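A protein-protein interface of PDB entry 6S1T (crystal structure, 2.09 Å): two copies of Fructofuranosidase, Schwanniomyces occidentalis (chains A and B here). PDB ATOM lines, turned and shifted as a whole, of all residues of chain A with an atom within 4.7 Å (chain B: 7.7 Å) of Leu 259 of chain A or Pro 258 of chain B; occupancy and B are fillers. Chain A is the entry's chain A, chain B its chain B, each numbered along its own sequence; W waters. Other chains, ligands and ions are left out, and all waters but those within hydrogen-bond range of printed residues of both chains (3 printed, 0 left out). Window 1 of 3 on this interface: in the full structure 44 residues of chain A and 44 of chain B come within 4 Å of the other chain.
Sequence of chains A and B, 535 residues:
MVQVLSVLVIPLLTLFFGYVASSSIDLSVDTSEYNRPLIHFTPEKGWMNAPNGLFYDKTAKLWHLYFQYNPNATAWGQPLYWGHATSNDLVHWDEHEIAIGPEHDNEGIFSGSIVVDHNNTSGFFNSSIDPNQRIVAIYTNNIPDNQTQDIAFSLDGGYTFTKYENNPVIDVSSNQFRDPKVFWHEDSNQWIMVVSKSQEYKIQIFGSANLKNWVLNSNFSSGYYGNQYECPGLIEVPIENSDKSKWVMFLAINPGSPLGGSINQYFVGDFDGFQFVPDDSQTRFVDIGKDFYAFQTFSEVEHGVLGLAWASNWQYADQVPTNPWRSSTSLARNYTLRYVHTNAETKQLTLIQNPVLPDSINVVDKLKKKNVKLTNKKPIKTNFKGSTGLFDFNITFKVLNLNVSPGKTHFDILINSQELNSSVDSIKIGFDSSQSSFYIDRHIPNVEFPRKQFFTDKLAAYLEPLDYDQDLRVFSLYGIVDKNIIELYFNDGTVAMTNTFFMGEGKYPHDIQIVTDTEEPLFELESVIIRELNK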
ATOM      1  N   SER A 257      14.212  -6.795  -6.821  1.00  0.00           N
ATOM      2  CA  SER A 257      15.676  -6.623  -7.033  1.00  0.00           C
ATOM      3  C   SER A 257      16.358  -7.963  -6.760  1.00  0.00           C
ATOM      4  O   SER A 257      15.986  -8.686  -5.825  1.00  0.00           O
ATOM      5  CB  SER A 257      16.265  -5.550  -6.159  1.00  0.00           C
ATOM      6  OG  SER A 257      17.679  -5.679  -6.061  1.00  0.00           O
ATOM      7  N   PRO A 258      17.412  -8.323  -7.524  1.00  0.00           N
ATOM      8  CA  PRO A 258      18.122  -9.566  -7.250  1.00  0.00           C
ATOM      9  C   PRO A 258      18.809  -9.482  -5.878  1.00  0.00           C
ATOM     10  O   PRO A 258      19.070 -10.515  -5.308  1.00  0.00           O
ATOM     11  CB  PRO A 258      19.108  -9.686  -8.417  1.00  0.00           C
ATOM     12  CG  PRO A 258      19.317  -8.251  -8.903  1.00  0.00           C
ATOM     13  CD  PRO A 258      18.020  -7.528  -8.607  1.00  0.00           C
ATOM     14  N   LEU A 259      19.031  -8.271  -5.354  1.00  0.00           N
ATOM     15  CA  LEU A 259      19.605  -8.060  -3.995  1.00  0.00           C
ATOM     16  C   LEU A 259      18.478  -7.981  -2.960  1.00  0.00           C
ATOM     17  O   LEU A 259      18.776  -7.798  -1.751  1.00  0.00           O
ATOM     18  CB  LEU A 259      20.454  -6.787  -4.001  1.00  0.00           C
ATOM     19  CG  LEU A 259      21.875  -6.956  -4.549  1.00  0.00           C
ATOM     20  CD1 LEU A 259      21.858  -7.656  -5.904  1.00  0.00           C
ATOM     21  CD2 LEU A 259      22.589  -5.614  -4.663  1.00  0.00           C
ATOM     22  N   GLY A 260      17.225  -8.125  -3.400  1.00  0.00           N
ATOM     23  CA  GLY A 260      16.050  -8.003  -2.521  1.00  0.00           C
ATOM     24  C   GLY A 260      15.585  -6.565  -2.420  1.00  0.00           C
ATOM     25  O   GLY A 260      16.412  -5.664  -2.076  1.00  0.00           O
ATOM     26  N   GLY A 261      14.311  -6.351  -2.742  1.00  0.00           N
ATOM     27  CA  GLY A 261      13.630  -5.059  -2.592  1.00  0.00           C
ATOM     28  C   GLY A 261      13.785  -4.221  -3.844  1.00  0.00           C
ATOM     29  O   GLY A 261      13.451  -4.698  -4.945  1.00  0.00           O
ATOM     30  N   ILE A 263      15.943  -1.389  -6.474  1.00  0.00           N
ATOM     31  CA  ILE A 263      17.272  -1.149  -7.104  1.00  0.00           C
ATOM     32  C   ILE A 263      17.091  -0.369  -8.417  1.00  0.00           C
ATOM     33  O   ILE A 263      15.983  -0.396  -8.982  1.00  0.00           O
ATOM     34  CB  ILE A 263      17.996  -2.498  -7.304  1.00  0.00           C
ATOM     35  CG1 ILE A 263      19.515  -2.336  -7.323  1.00  0.00           C
ATOM     36  CG2 ILE A 263      17.484  -3.213  -8.541  1.00  0.00           C
ATOM     37  CD1 ILE A 263      20.273  -3.642  -7.282  1.00  0.00           C
ATOM     38  N   PHE A 285      23.361  -2.614 -13.088  1.00  0.00           N
ATOM     39  CA  PHE A 285      22.785  -1.819 -11.974  1.00  0.00           C
ATOM     40  C   PHE A 285      23.596  -0.535 -11.784  1.00  0.00           C
ATOM     41  O   PHE A 285      24.824  -0.520 -12.040  1.00  0.00           O
ATOM     42  CB  PHE A 285      22.633  -2.679 -10.714  1.00  0.00           C
ATOM     43  CG  PHE A 285      21.723  -3.858 -10.941  1.00  0.00           C
ATOM     44  CD1 PHE A 285      20.364  -3.674 -11.169  1.00  0.00           C
ATOM     45  CD2 PHE A 285      22.233  -5.143 -11.001  1.00  0.00           C
ATOM     46  CE1 PHE A 285      19.535  -4.759 -11.411  1.00  0.00           C
ATOM     47  CE2 PHE A 285      21.405  -6.227 -11.254  1.00  0.00           C
ATOM     48  CZ  PHE A 285      20.061  -6.032 -11.456  1.00  0.00           C
ATOM     49  N   ILE A 288      25.192  -1.043  -6.498  1.00  0.00           N
ATOM     50  CA  ILE A 288      24.970  -2.456  -6.070  1.00  0.00           C
ATOM     51  C   ILE A 288      24.971  -2.549  -4.539  1.00  0.00           C
ATOM     52  O   ILE A 288      25.194  -3.653  -3.992  1.00  0.00           O
ATOM     53  CB  ILE A 288      25.970  -3.405  -6.746  1.00  0.00           C
ATOM     54  CG1 ILE A 288      27.417  -2.953  -6.542  1.00  0.00           C
ATOM     55  CG2 ILE A 288      25.601  -3.553  -8.211  1.00  0.00           C
ATOM     56  CD1 ILE A 288      28.425  -4.019  -6.870  1.00  0.00           C
ATOM     57  N   GLY A 289      24.694  -1.430  -3.866  1.00  0.00           N
ATOM     58  CA  GLY A 289      24.298  -1.434  -2.448  1.00  0.00           C
ATOM     59  C   GLY A 289      22.815  -1.738  -2.322  1.00  0.00           C
ATOM     60  O   GLY A 289      22.119  -1.811  -3.361  1.00  0.00           O
ATOM     61  N   LYS A 290      22.299  -1.869  -1.103  1.00  0.00           N
ATOM     62  CA  LYS A 290      20.853  -2.134  -0.921  1.00  0.00           C
ATOM     63  C   LYS A 290      20.045  -0.835  -0.951  1.00  0.00           C
ATOM     64  O   LYS A 290      18.828  -0.925  -1.174  1.00  0.00           O
ATOM     65  CB  LYS A 290      20.582  -2.832   0.408  1.00  0.00           C
ATOM     66  CG  LYS A 290      21.096  -4.263   0.508  1.00  0.00           C
ATOM     67  CD  LYS A 290      20.113  -5.311   0.031  1.00  0.00           C
ATOM     68  CE  LYS A 290      18.823  -5.316   0.825  1.00  0.00           C
ATOM     69  NZ  LYS A 290      17.915  -6.400   0.399  1.00  0.00           N
ATOM     70  N   THR A 456      20.006  -7.069   4.464  1.00  0.00           N
ATOM     71  CA  THR A 456      21.199  -7.861   4.082  1.00  0.00           C
ATOM     72  C   THR A 456      22.440  -7.219   4.718  1.00  0.00           C
ATOM     73  O   THR A 456      22.622  -6.007   4.573  1.00  0.00           O
ATOM     74  CB  THR A 456      21.319  -7.984   2.563  1.00  0.00           C
ATOM     75  OG1 THR A 456      20.020  -8.264   2.026  1.00  0.00           O
ATOM     76  CG2 THR A 456      22.342  -9.029   2.170  1.00  0.00           C
ATOM     77  N   TYR B 224      22.980 -10.757 -17.872  1.00  0.00           N
ATOM     78  CA  TYR B 224      23.970 -10.217 -16.910  1.00  0.00           C
ATOM     79  C   TYR B 224      25.345 -10.791 -17.249  1.00  0.00           C
ATOM     80  O   TYR B 224      25.546 -12.004 -17.060  1.00  0.00           O
ATOM     81  CB  TYR B 224      23.574 -10.552 -15.478  1.00  0.00           C
ATOM     82  CG  TYR B 224      24.057  -9.557 -14.461  1.00  0.00           C
ATOM     83  CD1 TYR B 224      23.389  -8.358 -14.279  1.00  0.00           C
ATOM     84  CD2 TYR B 224      25.150  -9.814 -13.655  1.00  0.00           C
ATOM     85  CE1 TYR B 224      23.797  -7.438 -13.329  1.00  0.00           C
ATOM     86  CE2 TYR B 224      25.572  -8.904 -12.692  1.00  0.00           C
ATOM     87  CZ  TYR B 224      24.890  -7.712 -12.528  1.00  0.00           C
ATOM     88  OH  TYR B 224      25.288  -6.814 -11.584  1.00  0.00           O
ATOM     89  N   GLY B 226      28.473 -10.118 -16.008  1.00  0.00           N
ATOM     90  CA  GLY B 226      29.456 -10.342 -14.931  1.00  0.00           C
ATOM     91  C   GLY B 226      30.879 -10.338 -15.479  1.00  0.00           C
ATOM     92  O   GLY B 226      31.201  -9.496 -16.356  1.00  0.00           O
ATOM     93  N   ILE B 253      27.608 -17.502 -15.072  1.00  0.00           N
ATOM     94  CA  ILE B 253      28.582 -16.379 -14.998  1.00  0.00           C
ATOM     95  C   ILE B 253      29.301 -16.440 -13.651  1.00  0.00           C
ATOM     96  O   ILE B 253      28.662 -16.737 -12.603  1.00  0.00           O
ATOM     97  CB  ILE B 253      27.919 -15.017 -15.260  1.00  0.00           C
ATOM     98  CG1 ILE B 253      26.788 -14.731 -14.273  1.00  0.00           C
ATOM     99  CG2 ILE B 253      27.449 -14.902 -16.702  1.00  0.00           C
ATOM    100  CD1 ILE B 253      26.540 -13.248 -14.085  1.00  0.00           C
ATOM    101  N   PRO B 255      33.301 -14.678 -11.865  1.00  0.00           N
ATOM    102  CA  PRO B 255      32.529 -14.052 -10.785  1.00  0.00           C
ATOM    103  C   PRO B 255      31.633 -12.919 -11.326  1.00  0.00           C
ATOM    104  O   PRO B 255      31.407 -12.867 -12.537  1.00  0.00           O
ATOM    105  CB  PRO B 255      33.631 -13.554  -9.844  1.00  0.00           C
ATOM    106  CG  PRO B 255      34.777 -13.227 -10.781  1.00  0.00           C
ATOM    107  CD  PRO B 255      34.726 -14.325 -11.819  1.00  0.00           C
ATOM    108  N   GLY B 256      31.083 -12.085 -10.435  1.00  0.00           N
ATOM    109  CA  GLY B 256      30.276 -10.902 -10.810  1.00  0.00           C
ATOM    110  C   GLY B 256      28.774 -11.147 -10.771  1.00  0.00           C
ATOM    111  O   GLY B 256      28.032 -10.277 -11.257  1.00  0.00           O
ATOM    112  N   SER B 257      28.303 -12.260 -10.203  1.00  0.00           N
ATOM    113  CA  SER B 257      26.857 -12.432  -9.898  1.00  0.00           C
ATOM    114  C   SER B 257      26.391 -11.236  -9.074  1.00  0.00           C
ATOM    115  O   SER B 257      27.112 -10.762  -8.194  1.00  0.00           O
ATOM    116  CB  SER B 257      26.568 -13.716  -9.162  1.00  0.00           C
ATOM    117  OG  SER B 257      25.285 -13.669  -8.549  1.00  0.00           O
ATOM    118  N   PRO B 258      25.159 -10.740  -9.294  1.00  0.00           N
ATOM    119  CA  PRO B 258      24.625  -9.653  -8.488  1.00  0.00           C
ATOM    120  C   PRO B 258      24.489 -10.106  -7.030  1.00  0.00           C
ATOM    121  O   PRO B 258      24.498  -9.257  -6.178  1.00  0.00           O
ATOM    122  CB  PRO B 258      23.257  -9.327  -9.115  1.00  0.00           C
ATOM    123  CG  PRO B 258      22.911 -10.526  -9.957  1.00  0.00           C
ATOM    124  CD  PRO B 258      24.218 -11.186 -10.328  1.00  0.00           C
ATOM    125  N   LEU B 259      24.397 -11.419  -6.781  1.00  0.00           N
ATOM    126  CA  LEU B 259      24.347 -11.969  -5.400  1.00  0.00           C
ATOM    127  C   LEU B 259      25.765 -12.239  -4.892  1.00  0.00           C
ATOM    128  O   LEU B 259      25.898 -12.735  -3.753  1.00  0.00           O
ATOM    129  CB  LEU B 259      23.511 -13.253  -5.388  1.00  0.00           C
ATOM    130  CG  LEU B 259      22.007 -13.066  -5.242  1.00  0.00           C
ATOM    131  CD1 LEU B 259      21.466 -12.239  -6.387  1.00  0.00           C
ATOM    132  CD2 LEU B 259      21.294 -14.409  -5.181  1.00  0.00           C
ATOM    133  N   GLY B 260      26.784 -11.928  -5.692  1.00  0.00           N
ATOM    134  CA  GLY B 260      28.189 -12.209  -5.349  1.00  0.00           C
ATOM    135  C   GLY B 260      28.596 -13.599  -5.789  1.00  0.00           C
ATOM    136  O   GLY B 260      27.917 -14.599  -5.407  1.00  0.00           O
ATOM    137  N   GLY B 261      29.655 -13.660  -6.589  1.00  0.00           N
ATOM    138  CA  GLY B 261      30.308 -14.913  -7.003  1.00  0.00           C
ATOM    139  C   GLY B 261      29.674 -15.457  -8.269  1.00  0.00           C
ATOM    140  O   GLY B 261      29.573 -14.722  -9.272  1.00  0.00           O
ATOM    141  N   SER B 262      29.156 -16.670  -8.162  1.00  0.00           N
ATOM    142  CA  SER B 262      28.726 -17.518  -9.294  1.00  0.00           C
ATOM    143  C   SER B 262      27.202 -17.662  -9.281  1.00  0.00           C
ATOM    144  O   SER B 262      26.601 -17.723  -8.186  1.00  0.00           O
ATOM    145  CB  SER B 262      29.446 -18.840  -9.203  1.00  0.00           C
ATOM    146  OG  SER B 262      29.371 -19.354  -7.878  1.00  0.00           O
ATOM    147  N   ILE B 263      26.593 -17.682 -10.466  1.00  0.00           N
ATOM    148  CA  ILE B 263      25.120 -17.829 -10.597  1.00  0.00           C
ATOM    149  C   ILE B 263      24.789 -18.290 -12.025  1.00  0.00           C
ATOM    150  O   ILE B 263      25.605 -18.057 -12.952  1.00  0.00           O
ATOM    151  CB  ILE B 263      24.419 -16.509 -10.206  1.00  0.00           C
ATOM    152  CG1 ILE B 263      22.986 -16.749  -9.723  1.00  0.00           C
ATOM    153  CG2 ILE B 263      24.478 -15.506 -11.349  1.00  0.00           C
ATOM    154  CD1 ILE B 263      22.327 -15.554  -9.080  1.00  0.00           C
ATOM    155  N   GLN B 265      21.817 -18.154 -15.182  1.00  0.00           N
ATOM    156  CA  GLN B 265      20.707 -17.358 -15.760  1.00  0.00           C
ATOM    157  C   GLN B 265      20.152 -18.090 -16.983  1.00  0.00           C
ATOM    158  O   GLN B 265      20.784 -19.067 -17.458  1.00  0.00           O
ATOM    159  CB  GLN B 265      21.167 -15.928 -16.067  1.00  0.00           C
ATOM    160  CG  GLN B 265      22.128 -15.808 -17.244  1.00  0.00           C
ATOM    161  CD  GLN B 265      22.712 -14.418 -17.364  1.00  0.00           C
ATOM    162  OE1 GLN B 265      22.021 -13.464 -17.702  1.00  0.00           O
ATOM    163  NE2 GLN B 265      23.998 -14.285 -17.094  1.00  0.00           N
ATOM    164  N   THR B 283      16.583 -10.297 -18.344  1.00  0.00           N
ATOM    165  CA  THR B 283      17.518 -11.127 -17.538  1.00  0.00           C
ATOM    166  C   THR B 283      16.745 -11.863 -16.434  1.00  0.00           C
ATOM    167  O   THR B 283      16.001 -11.191 -15.698  1.00  0.00           O
ATOM    168  CB  THR B 283      18.610 -10.249 -16.918  1.00  0.00           C
ATOM    169  OG1 THR B 283      19.380  -9.732 -18.000  1.00  0.00           O
ATOM    170  CG2 THR B 283      19.512 -10.987 -15.952  1.00  0.00           C
ATOM    171  N   PHE B 285      17.338 -15.350 -13.440  1.00  0.00           N
ATOM    172  CA  PHE B 285      18.245 -16.345 -12.813  1.00  0.00           C
ATOM    173  C   PHE B 285      17.484 -17.663 -12.632  1.00  0.00           C
ATOM    174  O   PHE B 285      16.262 -17.671 -12.426  1.00  0.00           O
ATOM    175  CB  PHE B 285      18.861 -15.760 -11.540  1.00  0.00           C
ATOM    176  CG  PHE B 285      19.700 -14.538 -11.826  1.00  0.00           C
ATOM    177  CD1 PHE B 285      20.856 -14.637 -12.578  1.00  0.00           C
ATOM    178  CD2 PHE B 285      19.298 -13.276 -11.400  1.00  0.00           C
ATOM    179  CE1 PHE B 285      21.596 -13.507 -12.896  1.00  0.00           C
ATOM    180  CE2 PHE B 285      20.057 -12.155 -11.690  1.00  0.00           C
ATOM    181  CZ  PHE B 285      21.214 -12.271 -12.426  1.00  0.00           C
ATOM    182  N   LYS B 290      22.663 -18.728  -3.227  1.00  0.00           N
ATOM    183  CA  LYS B 290      24.100 -18.482  -3.479  1.00  0.00           C
ATOM    184  C   LYS B 290      24.757 -19.709  -4.130  1.00  0.00           C
ATOM    185  O   LYS B 290      25.807 -19.517  -4.767  1.00  0.00           O
ATOM    186  CB  LYS B 290      24.781 -18.159  -2.146  1.00  0.00           C
ATOM    187  CG  LYS B 290      24.483 -16.777  -1.594  1.00  0.00           C
ATOM    188  CD  LYS B 290      25.267 -15.678  -2.287  1.00  0.00           C
ATOM    189  CE  LYS B 290      26.750 -15.730  -1.974  1.00  0.00           C
ATOM    190  NZ  LYS B 290      27.469 -14.530  -2.467  1.00  0.00           N
ATOM    191  N   THR B 456      27.015 -14.827   2.132  1.00  0.00           N
ATOM    192  CA  THR B 456      25.786 -14.031   2.371  1.00  0.00           C
ATOM    193  C   THR B 456      24.840 -14.857   3.254  1.00  0.00           C
ATOM    194  O   THR B 456      24.582 -16.015   2.907  1.00  0.00           O
ATOM    195  CB  THR B 456      25.129 -13.610   1.051  1.00  0.00           C
ATOM    196  OG1 THR B 456      26.147 -13.123   0.175  1.00  0.00           O
ATOM    197  CG2 THR B 456      24.050 -12.572   1.271  1.00  0.00           C
ATOM    198  N   LYS B 458      21.587 -13.711   4.533  1.00  0.00           N
ATOM    199  CA  LYS B 458      20.142 -13.389   4.393  1.00  0.00           C
ATOM    200  C   LYS B 458      19.810 -13.213   2.920  1.00  0.00           C
ATOM    201  O   LYS B 458      20.448 -12.365   2.263  1.00  0.00           O
ATOM    202  CB  LYS B 458      19.760 -12.120   5.152  1.00  0.00           C
ATOM    203  CG  LYS B 458      19.943 -12.174   6.659  1.00  0.00           C
ATOM    204  CD  LYS B 458      19.903 -10.785   7.202  1.00  0.00           C
ATOM    205  CE  LYS B 458      19.647 -10.646   8.681  1.00  0.00           C
ATOM    206  NZ  LYS B 458      19.831  -9.219   9.056  1.00  0.00           N
ATOM    207  N   LEU B 459      18.869 -14.013   2.436  1.00  0.00           N
ATOM    208  CA  LEU B 459      18.403 -13.969   1.032  1.00  0.00           C
ATOM    209  C   LEU B 459      16.874 -13.930   1.029  1.00  0.00           C
ATOM    210  O   LEU B 459      16.270 -14.511   1.940  1.00  0.00           O
ATOM    211  CB  LEU B 459      18.966 -15.195   0.319  1.00  0.00           C
ATOM    212  CG  LEU B 459      20.492 -15.283   0.369  1.00  0.00           C
ATOM    213  CD1 LEU B 459      20.962 -16.699   0.172  1.00  0.00           C
ATOM    214  CD2 LEU B 459      21.115 -14.356  -0.660  1.00  0.00           C
ATOM    215  N   ALA B 460      16.286 -13.219   0.072  1.00  0.00           N
ATOM    216  CA  ALA B 460      14.827 -13.059  -0.029  1.00  0.00           C
ATOM    217  C   ALA B 460      14.371 -13.452  -1.432  1.00  0.00           C
ATOM    218  O   ALA B 460      15.218 -13.495  -2.352  1.00  0.00           O
ATOM    219  CB  ALA B 460      14.442 -11.651   0.327  1.00  0.00           C
HETATM  220  O   HOH W   1      19.471 -10.493   0.390  1.00  0.00           O
HETATM  221  O   HOH W   2      25.600  -4.373 -12.500  1.00  0.00           O
HETATM  222  O   HOH W   3      15.425 -11.014  -3.805  1.00  0.00           O
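Pro 258 of chain A touches Leu 259 of chain B, and with the chains exchanged Leu 259 of chain A touches Pro 258 of chain B.
9 positions are printed for both chains.
Of the 4 pairs that touch across the chains among the printed residues, 2 have their exchanged pair printed and touching as well.
Water W2 lies within hydrogen-bond range of OH of Tyr 224 of chain B and N of Phe 285 of chain A.
Water W1 bridges the side-chain hydroxyl of Thr 456 of chain A and the backbone carbonyl oxygen of Lys 458 of chain B.
Water W3 lies within hydrogen-bond range of O of Ala 460 of chain B (2.9 Å), O of Ser 257 of chain A (3.1 Å) and N of Gly 260 of chain A (3.4 Å).
Of the 11 printed residues of chain A, 4 touch a printed residue of chain B.
Printed residues of chain A that touch a printed residue of chain B: Pro 258, Leu 259, Phe 285 and Thr 456.
Hydrophobic or aromatic side chains of chain A within 4 Å of the printed part of chain B: Leu 259 and Phe 285.
Printed residues of chain B that touch a printed residue of chain A: Tyr 224, Pro 258, Leu 259 and Lys 458.
Among the printed residues, 4 pairs touch across the chains.
Among the printed residues, no Asp or Glu carboxylate lies within 4 Å of a Lys or Arg side-chain nitrogen of the other chain.
Leu 259 of chain B touches Pro 258 of chain A (CD1 to O, 3.1 Å).
Leu 259 of chain A touches Pro 258 of chain B.
Phe 285 of chain A touches Tyr 224 of chain B.
CG2 of Thr 456 of chain A touches O of Lys 458 of chain B, at 3.8 Å.
Leu 259 of chain A touches just one residue of chain B: Pro 258.
Ile 263 of chain A touches none of the printed residues of chain B.
Printed residues of chain B within 4 Å of Thr 456 of chain A: Lys 458.
Pro 258 of chain B touches one residue of chain A.
Of the printed residues of chain A, Leu 259 of chain B touches Pro 258.
Ser 262 of chain B touches none of the printed residues of chain A.
Printed residues of chain A within 4 Å of Lys 458 of chain B: Thr 456.
The nearest residue of chain B that does not touch Leu 259 of chain A is Leu 259 of chain B (4.6 Å).
The nearest residue of chain A that does not touch Pro 258 of chain B is Pro 258 of chain A (4.1 Å).
OG of Ser 257 of chain A lies within hydrogen-bond range of N of Leu 259 of chain A (3.0 Å).
The backbone carbonyl oxygen of Leu 259 of chain A is in hydrogen-bond range of the side-chain amino group of Lys 290 of chain A (2.7 Å).
The side-chain amino group (NZ) of Lys 290 of chain A sits at hydrogen-bond distance from the side-chain hydroxyl (OG1) of Thr 456 of chain A (3.2 Å).
The backbone carbonyl oxygen of Tyr 224 of chain B lies within hydrogen-bond range of the side-chain amide nitrogen of Gln 265 of chain B (2.8 Å).
The side-chain hydroxyl (OG) of Ser 257 of chain B lies within hydrogen-bond range of the backbone NH (N) of Leu 259 of chain B (3.0 Å).
The backbone carbonyl oxygen (O) of Leu 259 of chain B is in hydrogen-bond range of the side-chain amino group (NZ) of Lys 290 of chain B, at 2.7 Å.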
